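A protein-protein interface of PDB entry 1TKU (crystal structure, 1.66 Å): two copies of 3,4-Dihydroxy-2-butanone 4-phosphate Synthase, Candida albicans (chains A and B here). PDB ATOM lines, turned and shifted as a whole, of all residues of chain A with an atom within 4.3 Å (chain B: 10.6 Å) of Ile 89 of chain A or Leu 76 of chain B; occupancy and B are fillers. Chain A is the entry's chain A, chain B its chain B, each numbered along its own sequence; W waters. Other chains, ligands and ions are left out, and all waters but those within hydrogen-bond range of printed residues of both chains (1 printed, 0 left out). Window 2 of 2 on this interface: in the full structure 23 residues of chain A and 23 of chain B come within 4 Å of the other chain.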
ATOM      1  N   LEU A  72      14.840   2.305  19.534  1.00  0.00           N
ATOM      2  CA  LEU A  72      15.275   3.636  19.948  1.00  0.00           C
ATOM      3  C   LEU A  72      14.170   4.599  19.524  1.00  0.00           C
ATOM      4  O   LEU A  72      14.259   5.240  18.475  1.00  0.00           O
ATOM      5  CB  LEU A  72      16.593   4.008  19.257  1.00  0.00           C
ATOM      6  CG  LEU A  72      17.809   3.162  19.642  1.00  0.00           C
ATOM      7  CD1 LEU A  72      18.999   3.530  18.764  1.00  0.00           C
ATOM      8  CD2 LEU A  72      18.129   3.378  21.117  1.00  0.00           C
ATOM      9  N   PRO A  73      13.107   4.709  20.337  1.00  0.00           N
ATOM     10  CA  PRO A  73      11.980   5.591  20.036  1.00  0.00           C
ATOM     11  C   PRO A  73      12.301   7.067  20.191  1.00  0.00           C
ATOM     12  O   PRO A  73      13.246   7.438  20.890  1.00  0.00           O
ATOM     13  CB  PRO A  73      10.922   5.136  21.032  1.00  0.00           C
ATOM     14  CG  PRO A  73      11.740   4.821  22.234  1.00  0.00           C
ATOM     15  CD  PRO A  73      12.912   4.048  21.639  1.00  0.00           C
ATOM     16  N   MET A  75      12.717  10.644  21.458  1.00  0.00           N
ATOM     17  CA  MET A  75      12.859  11.043  22.846  1.00  0.00           C
ATOM     18  C   MET A  75      11.525  11.536  23.391  1.00  0.00           C
ATOM     19  O   MET A  75      11.183  11.286  24.549  1.00  0.00           O
ATOM     20  CB  MET A  75      13.911  12.140  22.973  1.00  0.00           C
ATOM     21  CG  MET A  75      14.307  12.436  24.404  1.00  0.00           C
ATOM     22  SD  MET A  75      15.507  13.761  24.471  1.00  0.00           S
ATOM     23  CE  MET A  75      17.015  12.883  24.004  1.00  0.00           C
ATOM     24  N   THR A  88      16.281  10.488  19.526  1.00  0.00           N
ATOM     25  CA  THR A  88      15.687   9.284  20.083  1.00  0.00           C
ATOM     26  C   THR A  88      16.201   9.287  21.514  1.00  0.00           C
ATOM     27  O   THR A  88      16.982  10.168  21.891  1.00  0.00           O
ATOM     28  CB  THR A  88      16.203   7.993  19.398  1.00  0.00           C
ATOM     29  OG1 THR A  88      17.555   7.732  19.807  1.00  0.00           O
ATOM     30  CG2 THR A  88      16.148   8.131  17.889  1.00  0.00           C
ATOM     31  N   ILE A  89      15.755   8.335  22.322  1.00  0.00           N
ATOM     32  CA  ILE A  89      16.267   8.252  23.680  1.00  0.00           C
ATOM     33  C   ILE A  89      17.762   7.979  23.484  1.00  0.00           C
ATOM     34  O   ILE A  89      18.147   7.311  22.522  1.00  0.00           O
ATOM     35  CB  ILE A  89      15.616   7.086  24.458  1.00  0.00           C
ATOM     36  CG1 ILE A  89      16.143   7.065  25.895  1.00  0.00           C
ATOM     37  CG2 ILE A  89      15.911   5.763  23.761  1.00  0.00           C
ATOM     38  CD1 ILE A  89      15.401   6.108  26.809  1.00  0.00           C
ATOM     39  N   THR A  90      18.605   8.506  24.368  1.00  0.00           N
ATOM     40  CA  THR A  90      20.048   8.308  24.247  1.00  0.00           C
ATOM     41  C   THR A  90      20.450   6.889  24.634  1.00  0.00           C
ATOM     42  O   THR A  90      19.657   6.153  25.224  1.00  0.00           O
ATOM     43  CB  THR A  90      20.818   9.319  25.115  1.00  0.00           C
ATOM     44  OG1 THR A  90      20.444   9.159  26.490  1.00  0.00           O
ATOM     45  CG2 THR A  90      20.505  10.742  24.668  1.00  0.00           C
ATOM     46  N   CYS A  91      21.682   6.501  24.309  1.00  0.00           N
ATOM     47  CA  CYS A  91      22.129   5.148  24.620  1.00  0.00           C
ATOM     48  C   CYS A  91      23.639   4.932  24.637  1.00  0.00           C
ATOM     49  O   CYS A  91      24.410   5.758  24.151  1.00  0.00           O
ATOM     50  CB  CYS A  91      21.518   4.172  23.609  1.00  0.00           C
ATOM     51  SG  CYS A  91      22.217   4.332  21.935  1.00  0.00           S
ATOM     52  N   LYS A 125      19.911   2.294  28.045  1.00  0.00           N
ATOM     53  CA  LYS A 125      19.254   3.575  27.825  1.00  0.00           C
ATOM     54  C   LYS A 125      18.770   4.124  29.165  1.00  0.00           C
ATOM     55  O   LYS A 125      18.215   3.385  29.977  1.00  0.00           O
ATOM     56  CB  LYS A 125      18.073   3.395  26.866  1.00  0.00           C
ATOM     57  CG  LYS A 125      18.490   2.940  25.469  1.00  0.00           C
ATOM     58  CD  LYS A 125      17.306   2.465  24.644  1.00  0.00           C
ATOM     59  CE  LYS A 125      16.736   1.170  25.198  1.00  0.00           C
ATOM     60  NZ  LYS A 125      15.659   0.616  24.337  1.00  0.00           N
ATOM     61  N   PRO A 126      18.992   5.423  29.423  1.00  0.00           N
ATOM     62  CA  PRO A 126      19.664   6.407  28.564  1.00  0.00           C
ATOM     63  C   PRO A 126      21.173   6.187  28.521  1.00  0.00           C
ATOM     64  O   PRO A 126      21.711   5.347  29.248  1.00  0.00           O
ATOM     65  CB  PRO A 126      19.291   7.736  29.217  1.00  0.00           C
ATOM     66  CG  PRO A 126      19.239   7.371  30.664  1.00  0.00           C
ATOM     67  CD  PRO A 126      18.469   6.072  30.638  1.00  0.00           C
ATOM     68  N   PRO A 131      21.252   9.247  19.241  1.00  0.00           N
ATOM     69  CA  PRO A 131      20.852   8.758  17.918  1.00  0.00           C
ATOM     70  C   PRO A 131      19.815   9.709  17.319  1.00  0.00           C
ATOM     71  O   PRO A 131      19.044  10.333  18.052  1.00  0.00           O
ATOM     72  CB  PRO A 131      20.242   7.381  18.215  1.00  0.00           C
ATOM     73  CG  PRO A 131      20.858   6.987  19.533  1.00  0.00           C
ATOM     74  CD  PRO A 131      20.865   8.290  20.291  1.00  0.00           C
ATOM     75  N   TYR B  57      29.293  17.165  26.438  1.00  0.00           N
ATOM     76  CA  TYR B  57      27.989  16.611  26.805  1.00  0.00           C
ATOM     77  C   TYR B  57      27.612  17.363  28.082  1.00  0.00           C
ATOM     78  O   TYR B  57      27.617  16.799  29.179  1.00  0.00           O
ATOM     79  CB  TYR B  57      28.132  15.104  27.079  1.00  0.00           C
ATOM     80  CG  TYR B  57      26.886  14.279  26.819  1.00  0.00           C
ATOM     81  CD1 TYR B  57      26.347  14.179  25.536  1.00  0.00           C
ATOM     82  CD2 TYR B  57      26.265  13.573  27.848  1.00  0.00           C
ATOM     83  CE1 TYR B  57      25.222  13.400  25.283  1.00  0.00           C
ATOM     84  CE2 TYR B  57      25.135  12.782  27.604  1.00  0.00           C
ATOM     85  CZ  TYR B  57      24.620  12.701  26.321  1.00  0.00           C
ATOM     86  OH  TYR B  57      23.505  11.930  26.070  1.00  0.00           O
ATOM     87  N   LEU B  72      10.129  18.506  33.501  1.00  0.00           N
ATOM     88  CA  LEU B  72      11.256  17.845  32.849  1.00  0.00           C
ATOM     89  C   LEU B  72      11.328  16.444  33.447  1.00  0.00           C
ATOM     90  O   LEU B  72      12.119  16.184  34.354  1.00  0.00           O
ATOM     91  CB  LEU B  72      12.556  18.602  33.130  1.00  0.00           C
ATOM     92  CG  LEU B  72      12.657  20.001  32.521  1.00  0.00           C
ATOM     93  CD1 LEU B  72      13.910  20.703  33.032  1.00  0.00           C
ATOM     94  CD2 LEU B  72      12.673  19.891  31.004  1.00  0.00           C
ATOM     95  N   PRO B  73      10.496  15.520  32.943  1.00  0.00           N
ATOM     96  CA  PRO B  73      10.457  14.140  33.430  1.00  0.00           C
ATOM     97  C   PRO B  73      11.673  13.317  33.034  1.00  0.00           C
ATOM     98  O   PRO B  73      12.383  13.661  32.086  1.00  0.00           O
ATOM     99  CB  PRO B  73       9.177  13.602  32.805  1.00  0.00           C
ATOM    100  CG  PRO B  73       9.169  14.274  31.475  1.00  0.00           C
ATOM    101  CD  PRO B  73       9.556  15.704  31.821  1.00  0.00           C
ATOM    102  N   PRO B  74      11.937  12.221  33.764  1.00  0.00           N
ATOM    103  CA  PRO B  74      13.083  11.370  33.443  1.00  0.00           C
ATOM    104  C   PRO B  74      13.003  10.998  31.967  1.00  0.00           C
ATOM    105  O   PRO B  74      11.915  10.793  31.428  1.00  0.00           O
ATOM    106  CB  PRO B  74      12.879  10.162  34.354  1.00  0.00           C
ATOM    107  CG  PRO B  74      12.216  10.762  35.553  1.00  0.00           C
ATOM    108  CD  PRO B  74      11.202  11.691  34.928  1.00  0.00           C
ATOM    109  N   MET B  75      14.149  10.921  31.305  1.00  0.00           N
ATOM    110  CA  MET B  75      14.156  10.585  29.894  1.00  0.00           C
ATOM    111  C   MET B  75      13.494   9.231  29.671  1.00  0.00           C
ATOM    112  O   MET B  75      12.814   9.019  28.664  1.00  0.00           O
ATOM    113  CB  MET B  75      15.585  10.556  29.368  1.00  0.00           C
ATOM    114  CG  MET B  75      15.668  10.521  27.862  1.00  0.00           C
ATOM    115  SD  MET B  75      17.373  10.429  27.337  1.00  0.00           S
ATOM    116  CE  MET B  75      17.876  12.164  27.471  1.00  0.00           C
ATOM    117  N   LEU B  76      13.699   8.317  30.614  1.00  0.00           N
ATOM    118  CA  LEU B  76      13.107   6.990  30.525  1.00  0.00           C
ATOM    119  C   LEU B  76      12.111   6.821  31.666  1.00  0.00           C
ATOM    120  O   LEU B  76      12.495   6.763  32.834  1.00  0.00           O
ATOM    121  CB  LEU B  76      14.197   5.914  30.613  1.00  0.00           C
ATOM    122  CG  LEU B  76      13.810   4.465  30.286  1.00  0.00           C
ATOM    123  CD1 LEU B  76      12.868   3.903  31.345  1.00  0.00           C
ATOM    124  CD2 LEU B  76      13.164   4.418  28.909  1.00  0.00           C
ATOM    125  N   ALA B  77      10.831   6.745  31.316  1.00  0.00           N
ATOM    126  CA  ALA B  77       9.767   6.587  32.301  1.00  0.00           C
ATOM    127  C   ALA B  77       9.874   5.242  33.011  1.00  0.00           C
ATOM    128  O   ALA B  77       9.039   4.908  33.853  1.00  0.00           O
ATOM    129  CB  ALA B  77       8.407   6.714  31.620  1.00  0.00           C
ATOM    130  N   GLY B  84      21.934   6.279  38.441  1.00  0.00           N
ATOM    131  CA  GLY B  84      22.990   6.157  37.447  1.00  0.00           C
ATOM    132  C   GLY B  84      23.086   7.306  36.456  1.00  0.00           C
ATOM    133  O   GLY B  84      23.482   7.116  35.299  1.00  0.00           O
ATOM    134  N   THR B  85      22.766   8.506  36.921  1.00  0.00           N
ATOM    135  CA  THR B  85      22.778   9.720  36.103  1.00  0.00           C
ATOM    136  C   THR B  85      21.349   9.776  35.600  1.00  0.00           C
ATOM    137  O   THR B  85      20.999   9.152  34.597  1.00  0.00           O
ATOM    138  CB  THR B  85      23.761   9.676  34.893  1.00  0.00           C
ATOM    139  OG1 THR B  85      25.091   9.402  35.351  1.00  0.00           O
ATOM    140  CG2 THR B  85      23.764  11.018  34.181  1.00  0.00           C
ATOM    141  N   ALA B  86      20.517  10.504  36.336  1.00  0.00           N
ATOM    142  CA  ALA B  86      19.105  10.645  36.014  1.00  0.00           C
ATOM    143  C   ALA B  86      18.841  11.732  34.982  1.00  0.00           C
ATOM    144  O   ALA B  86      18.477  12.853  35.332  1.00  0.00           O
ATOM    145  CB  ALA B  86      18.316  10.949  37.288  1.00  0.00           C
ATOM    146  N   TYR B  87      19.007  11.398  33.709  1.00  0.00           N
ATOM    147  CA  TYR B  87      18.753  12.365  32.656  1.00  0.00           C
ATOM    148  C   TYR B  87      17.259  12.612  32.498  1.00  0.00           C
ATOM    149  O   TYR B  87      16.449  11.699  32.649  1.00  0.00           O
ATOM    150  CB  TYR B  87      19.278  11.866  31.309  1.00  0.00           C
ATOM    151  CG  TYR B  87      20.759  11.604  31.244  1.00  0.00           C
ATOM    152  CD1 TYR B  87      21.268  10.317  31.417  1.00  0.00           C
ATOM    153  CD2 TYR B  87      21.652  12.636  30.965  1.00  0.00           C
ATOM    154  CE1 TYR B  87      22.631  10.064  31.308  1.00  0.00           C
ATOM    155  CE2 TYR B  87      23.019  12.396  30.856  1.00  0.00           C
ATOM    156  CZ  TYR B  87      23.501  11.108  31.028  1.00  0.00           C
ATOM    157  OH  TYR B  87      24.853  10.876  30.939  1.00  0.00           O
ATOM    158  N   THR B  88      16.897  13.852  32.202  1.00  0.00           N
ATOM    159  CA  THR B  88      15.504  14.183  31.956  1.00  0.00           C
ATOM    160  C   THR B  88      15.468  14.369  30.444  1.00  0.00           C
ATOM    161  O   THR B  88      16.510  14.269  29.779  1.00  0.00           O
ATOM    162  CB  THR B  88      15.091  15.520  32.613  1.00  0.00           C
ATOM    163  OG1 THR B  88      15.694  16.618  31.911  1.00  0.00           O
ATOM    164  CG2 THR B  88      15.523  15.557  34.070  1.00  0.00           C
ATOM    165  N   ILE B  89      14.287  14.604  29.886  1.00  0.00           N
ATOM    166  CA  ILE B  89      14.207  14.867  28.458  1.00  0.00           C
ATOM    167  C   ILE B  89      15.035  16.141  28.283  1.00  0.00           C
ATOM    168  O   ILE B  89      15.064  16.992  29.171  1.00  0.00           O
ATOM    169  CB  ILE B  89      12.746  15.115  28.008  1.00  0.00           C
ATOM    170  CG1 ILE B  89      11.965  13.794  27.973  1.00  0.00           C
ATOM    171  CG2 ILE B  89      12.717  15.731  26.613  1.00  0.00           C
ATOM    172  CD1 ILE B  89      11.795  13.119  29.313  1.00  0.00           C
ATOM    173  N   THR B  90      15.728  16.271  27.157  1.00  0.00           N
ATOM    174  CA  THR B  90      16.561  17.448  26.924  1.00  0.00           C
ATOM    175  C   THR B  90      15.713  18.682  26.617  1.00  0.00           C
ATOM    176  O   THR B  90      14.515  18.567  26.350  1.00  0.00           O
ATOM    177  CB  THR B  90      17.551  17.200  25.775  1.00  0.00           C
ATOM    178  OG1 THR B  90      16.831  16.838  24.593  1.00  0.00           O
ATOM    179  CG2 THR B  90      18.511  16.070  26.144  1.00  0.00           C
ATOM    180  N   PRO B 126      12.442  18.151  22.562  1.00  0.00           N
ATOM    181  CA  PRO B 126      13.797  18.019  23.109  1.00  0.00           C
ATOM    182  C   PRO B 126      14.655  19.246  22.797  1.00  0.00           C
ATOM    183  O   PRO B 126      14.220  20.153  22.080  1.00  0.00           O
ATOM    184  CB  PRO B 126      14.315  16.755  22.428  1.00  0.00           C
ATOM    185  CG  PRO B 126      13.651  16.818  21.093  1.00  0.00           C
ATOM    186  CD  PRO B 126      12.235  17.198  21.456  1.00  0.00           C
ATOM    187  N   LEU B 130      21.186  18.947  28.694  1.00  0.00           N
ATOM    188  CA  LEU B 130      20.789  17.728  29.400  1.00  0.00           C
ATOM    189  C   LEU B 130      20.566  17.958  30.898  1.00  0.00           C
ATOM    190  O   LEU B 130      21.508  17.922  31.684  1.00  0.00           O
ATOM    191  CB  LEU B 130      21.869  16.655  29.221  1.00  0.00           C
ATOM    192  CG  LEU B 130      22.154  16.144  27.805  1.00  0.00           C
ATOM    193  CD1 LEU B 130      23.654  16.144  27.556  1.00  0.00           C
ATOM    194  CD2 LEU B 130      21.590  14.741  27.628  1.00  0.00           C
ATOM    195  N   PRO B 131      19.313  18.199  31.313  1.00  0.00           N
ATOM    196  CA  PRO B 131      19.071  18.417  32.742  1.00  0.00           C
ATOM    197  C   PRO B 131      19.194  17.082  33.480  1.00  0.00           C
ATOM    198  O   PRO B 131      18.889  16.028  32.919  1.00  0.00           O
ATOM    199  CB  PRO B 131      17.637  18.960  32.779  1.00  0.00           C
ATOM    200  CG  PRO B 131      17.429  19.526  31.399  1.00  0.00           C
ATOM    201  CD  PRO B 131      18.107  18.497  30.529  1.00  0.00           C
ATOM    202  N   ARG B 133      18.445  15.025  37.334  1.00  0.00           N
ATOM    203  CA  ARG B 133      17.666  15.101  38.562  1.00  0.00           C
ATOM    204  C   ARG B 133      18.442  14.613  39.782  1.00  0.00           C
ATOM    205  O   ARG B 133      18.682  13.416  39.936  1.00  0.00           O
ATOM    206  CB  ARG B 133      16.372  14.287  38.417  1.00  0.00           C
ATOM    207  CG  ARG B 133      15.449  14.779  37.311  1.00  0.00           C
ATOM    208  CD  ARG B 133      14.131  14.010  37.282  1.00  0.00           C
ATOM    209  NE  ARG B 133      13.351  14.249  38.494  1.00  0.00           N
ATOM    210  CZ  ARG B 133      12.113  13.810  38.695  1.00  0.00           C
ATOM    211  NH1 ARG B 133      11.495  13.102  37.759  1.00  0.00           N
ATOM    212  NH2 ARG B 133      11.491  14.079  39.834  1.00  0.00           N
HETATM  213  O   HOH W   1      21.551  11.219  27.927  1.00  0.00           O
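Met 75 of chain A touches its own counterpart, Met 75 of chain B. Met 75 of chain A touches Thr 90 of chain B, and with the chains exchanged Thr 90 of chain A touches Met 75 of chain B. Met 75 of chain A touches Pro 126 of chain B, and with the chains exchanged Pro 126 of chain A touches Met 75 of chain B. Ile 89 of chain A touches Met 75 of chain B, but with the chains exchanged Met 75 of chain A does not touch Ile 89 of chain B (4.03 Å). Positions printed for both chains: 72, 73, 75, 88, 89, 90, 126 and 131. Of the 9 pairs that touch across the chains among the printed residues, 5 have their exchanged pair printed and touching as well.
The side-chain sulfur of Met 75 of chain A lies within hydrogen-bond range of the side-chain hydroxyl of Thr 90 of chain B, 3.4 Å away. The side-chain hydroxyl of Thr 90 of chain A sits at hydrogen-bond distance from the side-chain sulfur of Met 75 of chain B, 3.4 Å away.
Of chain A, only Ile 89 (3.5 Å) comes within 4 Å of Leu 76 of chain B. Printed residues of chain B within 4 Å of Met 75 of chain A: Met 75, Thr 90 and Pro 126. No residue of chain B comes within 4 Å of Thr 88 of chain A. Of the printed residues of chain B, Thr 90 of chain A touches Tyr 57 and Met 75. No residue of chain B comes within 4 Å of Lys 125 of chain A. Of the printed residues of chain A, Tyr 87 of chain B touches Pro 126 (3.7 Å). Of the printed residues of chain A, Met 75 of chain B touches Met 75 (3.6 Å), Ile 89 (3.9 Å), Thr 90 (3.4 Å) and Pro 126 (3.8 Å). Ala 86 of chain B touches none of the printed residues of chain A. Pro 73 of chain B touches none of the printed residues of chain A.
Water W1 bridges OG1 of Thr 90 of chain A and OH of Tyr 57 of chain B.
The backbone carbonyl oxygen (O) of Pro 73 of chain A is in hydrogen-bond range of the backbone NH (N) of Ile 89 of chain A, at 3.0 Å. N of Met 75 of chain B is in hydrogen-bond range of O of Tyr 87 of chain B (2.8 Å).
Met 75 of chain A touches Met 75 of chain B. Pro 126 of chain B touches Met 75 of chain A. CG1 of Ile 89 of chain A touches SD of Met 75 of chain B, 3.9 Å away. Ile 89 of chain A touches Leu 76 of chain B. CG2 of Thr 90 of chain A touches OH of Tyr 57 of chain B, 3.5 Å away. SD of Met 75 of chain B touches CB of Pro 126 of chain A (3.8 Å). Pro 126 of chain A touches Tyr 87 of chain B (CG to CD1, 3.7 Å).
Of the 18 printed residues of chain B, 6 touch a printed residue of chain A. Among the printed residues, no Asp or Glu carboxylate lies within 4 Å of a Lys or Arg side-chain nitrogen of the other chain.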
